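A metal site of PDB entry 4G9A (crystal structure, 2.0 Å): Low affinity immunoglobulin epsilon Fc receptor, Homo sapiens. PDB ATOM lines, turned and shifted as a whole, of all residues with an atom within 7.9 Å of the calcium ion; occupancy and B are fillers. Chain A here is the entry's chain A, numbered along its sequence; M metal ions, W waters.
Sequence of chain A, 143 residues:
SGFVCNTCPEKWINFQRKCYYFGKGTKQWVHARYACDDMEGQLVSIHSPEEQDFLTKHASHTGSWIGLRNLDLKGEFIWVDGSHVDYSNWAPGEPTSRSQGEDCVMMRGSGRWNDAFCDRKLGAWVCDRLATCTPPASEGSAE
Water W1 binds the calcium ion (2.4 Å).
OE2 of Glu 94 binds the calcium ion, 2.5 Å away.
Water W2 binds the calcium ion (2.6 Å).
OD2 of Asp 115 is bound to the calcium ion, at 2.6 Å.
OG1 of Thr 96 is bound to the calcium ion (2.6 Å).
The calcium ion is bound by the side-chain carboxylate (OE1) of Glu 94 (2.7 Å).
The calcium ion has six donor atoms within binding distance.
Water W1 lies within hydrogen-bond range of O of Asp 115 (2.7 Å) and ND2 of Asn 114 (3.5 Å).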
ATOM      1  N   TRP A  90     -22.295 -12.136  -8.658  1.00  0.00           N
ATOM      2  CA  TRP A  90     -21.167 -12.189  -9.577  1.00  0.00           C
ATOM      3  C   TRP A  90     -21.579 -12.597 -10.975  1.00  0.00           C
ATOM      4  O   TRP A  90     -22.426 -13.478 -11.161  1.00  0.00           O
ATOM      5  CB  TRP A  90     -20.122 -13.199  -9.080  1.00  0.00           C
ATOM      6  CG  TRP A  90     -19.456 -12.822  -7.777  1.00  0.00           C
ATOM      7  CD1 TRP A  90     -19.650 -13.406  -6.567  1.00  0.00           C
ATOM      8  CD2 TRP A  90     -18.480 -11.781  -7.587  1.00  0.00           C
ATOM      9  NE1 TRP A  90     -18.865 -12.789  -5.616  1.00  0.00           N
ATOM     10  CE2 TRP A  90     -18.132 -11.796  -6.211  1.00  0.00           C
ATOM     11  CE3 TRP A  90     -17.870 -10.847  -8.426  1.00  0.00           C
ATOM     12  CZ2 TRP A  90     -17.208 -10.900  -5.666  1.00  0.00           C
ATOM     13  CZ3 TRP A  90     -16.940  -9.963  -7.883  1.00  0.00           C
ATOM     14  CH2 TRP A  90     -16.623  -9.997  -6.516  1.00  0.00           C
ATOM     15  N   PRO A  92     -20.897 -14.497 -14.546  1.00  0.00           N
ATOM     16  CA  PRO A  92     -20.324 -15.818 -14.770  1.00  0.00           C
ATOM     17  C   PRO A  92     -18.803 -15.763 -14.859  1.00  0.00           C
ATOM     18  O   PRO A  92     -18.240 -14.946 -15.606  1.00  0.00           O
ATOM     19  CB  PRO A  92     -20.920 -16.239 -16.112  1.00  0.00           C
ATOM     20  CG  PRO A  92     -22.179 -15.483 -16.211  1.00  0.00           C
ATOM     21  CD  PRO A  92     -21.919 -14.155 -15.548  1.00  0.00           C
ATOM     22  N   GLY A  93     -18.121 -16.600 -14.081  1.00  0.00           N
ATOM     23  CA  GLY A  93     -16.680 -16.650 -14.093  1.00  0.00           C
ATOM     24  C   GLY A  93     -16.023 -15.653 -13.147  1.00  0.00           C
ATOM     25  O   GLY A  93     -14.809 -15.601 -13.062  1.00  0.00           O
ATOM     26  N   GLU A  94     -16.834 -14.868 -12.448  1.00  0.00           N
ATOM     27  CA  GLU A  94     -16.306 -13.893 -11.492  1.00  0.00           C
ATOM     28  C   GLU A  94     -16.555 -14.328 -10.048  1.00  0.00           C
ATOM     29  O   GLU A  94     -17.524 -15.020  -9.776  1.00  0.00           O
ATOM     30  CB  GLU A  94     -16.938 -12.519 -11.723  1.00  0.00           C
ATOM     31  CG  GLU A  94     -16.632 -11.943 -13.084  1.00  0.00           C
ATOM     32  CD  GLU A  94     -15.179 -11.576 -13.230  1.00  0.00           C
ATOM     33  OE1 GLU A  94     -14.666 -10.866 -12.342  1.00  0.00           O
ATOM     34  OE2 GLU A  94     -14.543 -12.002 -14.210  1.00  0.00           O
ATOM     35  N   PRO A  95     -15.666 -13.925  -9.133  1.00  0.00           N
ATOM     36  CA  PRO A  95     -14.436 -13.164  -9.417  1.00  0.00           C
ATOM     37  C   PRO A  95     -13.354 -14.082  -9.990  1.00  0.00           C
ATOM     38  O   PRO A  95     -13.452 -15.292  -9.879  1.00  0.00           O
ATOM     39  CB  PRO A  95     -14.016 -12.644  -8.035  1.00  0.00           C
ATOM     40  CG  PRO A  95     -14.527 -13.669  -7.091  1.00  0.00           C
ATOM     41  CD  PRO A  95     -15.793 -14.248  -7.697  1.00  0.00           C
ATOM     42  N   THR A  96     -12.335 -13.494 -10.607  1.00  0.00           N
ATOM     43  CA  THR A  96     -11.273 -14.294 -11.199  1.00  0.00           C
ATOM     44  C   THR A  96     -10.447 -14.988 -10.118  1.00  0.00           C
ATOM     45  O   THR A  96     -10.042 -14.358  -9.135  1.00  0.00           O
ATOM     46  CB  THR A  96     -10.367 -13.453 -12.103  1.00  0.00           C
ATOM     47  OG1 THR A  96     -11.109 -13.038 -13.256  1.00  0.00           O
ATOM     48  CG2 THR A  96      -9.165 -14.269 -12.573  1.00  0.00           C
ATOM     49  N   SER A  97     -10.229 -16.280 -10.307  1.00  0.00           N
ATOM     50  CA  SER A  97      -9.530 -17.123  -9.340  1.00  0.00           C
ATOM     51  C   SER A  97      -8.028 -16.890  -9.382  1.00  0.00           C
ATOM     52  O   SER A  97      -7.258 -17.825  -9.599  1.00  0.00           O
ATOM     53  CB  SER A  97      -9.814 -18.600  -9.591  1.00  0.00           C
ATOM     54  OG  SER A  97     -11.190 -18.897  -9.446  1.00  0.00           O
ATOM     55  N   GLN A 100      -4.354 -11.120  -8.311  1.00  0.00           N
ATOM     56  CA  GLN A 100      -3.505 -10.410  -9.273  1.00  0.00           C
ATOM     57  C   GLN A 100      -3.718  -8.890  -9.308  1.00  0.00           C
ATOM     58  O   GLN A 100      -3.453  -8.244 -10.325  1.00  0.00           O
ATOM     59  CB  GLN A 100      -3.635 -11.027 -10.673  1.00  0.00           C
ATOM     60  CG  GLN A 100      -5.005 -10.897 -11.302  1.00  0.00           C
ATOM     61  CD  GLN A 100      -5.036 -11.431 -12.739  1.00  0.00           C
ATOM     62  OE1 GLN A 100      -4.009 -11.533 -13.399  1.00  0.00           O
ATOM     63  NE2 GLN A 100      -6.229 -11.770 -13.201  1.00  0.00           N
ATOM     64  N   GLU A 102      -6.533  -7.023  -8.982  1.00  0.00           N
ATOM     65  CA  GLU A 102      -7.803  -6.441  -9.385  1.00  0.00           C
ATOM     66  C   GLU A 102      -8.722  -6.540  -8.175  1.00  0.00           C
ATOM     67  O   GLU A 102      -9.506  -7.475  -8.044  1.00  0.00           O
ATOM     68  CB  GLU A 102      -8.372  -7.152 -10.613  1.00  0.00           C
ATOM     69  CG  GLU A 102      -7.363  -7.144 -11.749  1.00  0.00           C
ATOM     70  CD  GLU A 102      -7.903  -7.697 -13.033  1.00  0.00           C
ATOM     71  OE1 GLU A 102      -9.083  -7.439 -13.343  1.00  0.00           O
ATOM     72  OE2 GLU A 102      -7.146  -8.386 -13.744  1.00  0.00           O
ATOM     73  N   TRP A 113     -21.804  -8.432 -11.069  1.00  0.00           N
ATOM     74  CA  TRP A 113     -20.533  -7.886 -10.595  1.00  0.00           C
ATOM     75  C   TRP A 113     -19.309  -8.523 -11.268  1.00  0.00           C
ATOM     76  O   TRP A 113     -19.332  -9.683 -11.649  1.00  0.00           O
ATOM     77  CB  TRP A 113     -20.385  -8.110  -9.084  1.00  0.00           C
ATOM     78  CG  TRP A 113     -21.560  -7.750  -8.224  1.00  0.00           C
ATOM     79  CD1 TRP A 113     -22.607  -6.939  -8.532  1.00  0.00           C
ATOM     80  CD2 TRP A 113     -21.783  -8.198  -6.881  1.00  0.00           C
ATOM     81  NE1 TRP A 113     -23.482  -6.866  -7.475  1.00  0.00           N
ATOM     82  CE2 TRP A 113     -22.995  -7.621  -6.436  1.00  0.00           C
ATOM     83  CE3 TRP A 113     -21.071  -9.037  -6.007  1.00  0.00           C
ATOM     84  CZ2 TRP A 113     -23.520  -7.863  -5.165  1.00  0.00           C
ATOM     85  CZ3 TRP A 113     -21.600  -9.272  -4.748  1.00  0.00           C
ATOM     86  CH2 TRP A 113     -22.806  -8.687  -4.336  1.00  0.00           C
ATOM     87  N   ASN A 114     -18.231  -7.744 -11.370  1.00  0.00           N
ATOM     88  CA  ASN A 114     -16.926  -8.270 -11.746  1.00  0.00           C
ATOM     89  C   ASN A 114     -15.829  -7.525 -11.012  1.00  0.00           C
ATOM     90  O   ASN A 114     -15.982  -6.362 -10.667  1.00  0.00           O
ATOM     91  CB  ASN A 114     -16.715  -8.232 -13.266  1.00  0.00           C
ATOM     92  CG  ASN A 114     -16.674  -6.823 -13.823  1.00  0.00           C
ATOM     93  OD1 ASN A 114     -17.682  -6.286 -14.244  1.00  0.00           O
ATOM     94  ND2 ASN A 114     -15.479  -6.230 -13.856  1.00  0.00           N
ATOM     95  N   ASP A 115     -14.719  -8.207 -10.731  1.00  0.00           N
ATOM     96  CA  ASP A 115     -13.605  -7.531 -10.106  1.00  0.00           C
ATOM     97  C   ASP A 115     -12.915  -6.679 -11.159  1.00  0.00           C
ATOM     98  O   ASP A 115     -13.160  -6.849 -12.361  1.00  0.00           O
ATOM     99  CB  ASP A 115     -12.628  -8.502  -9.438  1.00  0.00           C
ATOM    100  CG  ASP A 115     -12.113  -9.565 -10.400  1.00  0.00           C
ATOM    101  OD1 ASP A 115     -11.805 -10.679  -9.951  1.00  0.00           O
ATOM    102  OD2 ASP A 115     -12.014  -9.266 -11.605  1.00  0.00           O
ATOM    103  N   ALA A 116     -12.079  -5.748 -10.718  1.00  0.00           N
ATOM    104  CA  ALA A 116     -11.416  -4.831 -11.653  1.00  0.00           C
ATOM    105  C   ALA A 116     -10.236  -4.166 -10.989  1.00  0.00           C
ATOM    106  O   ALA A 116     -10.131  -4.155  -9.768  1.00  0.00           O
ATOM    107  CB  ALA A 116     -12.411  -3.787 -12.146  1.00  0.00           C
HETATM  108 CA    CA M   1     -12.368 -10.782 -13.706  1.00  0.00          CA
HETATM  109  O   HOH W   1     -12.934  -8.532 -14.410  1.00  0.00           O
HETATM  110  O   HOH W   2     -11.962 -11.470 -16.163  1.00  0.00           O
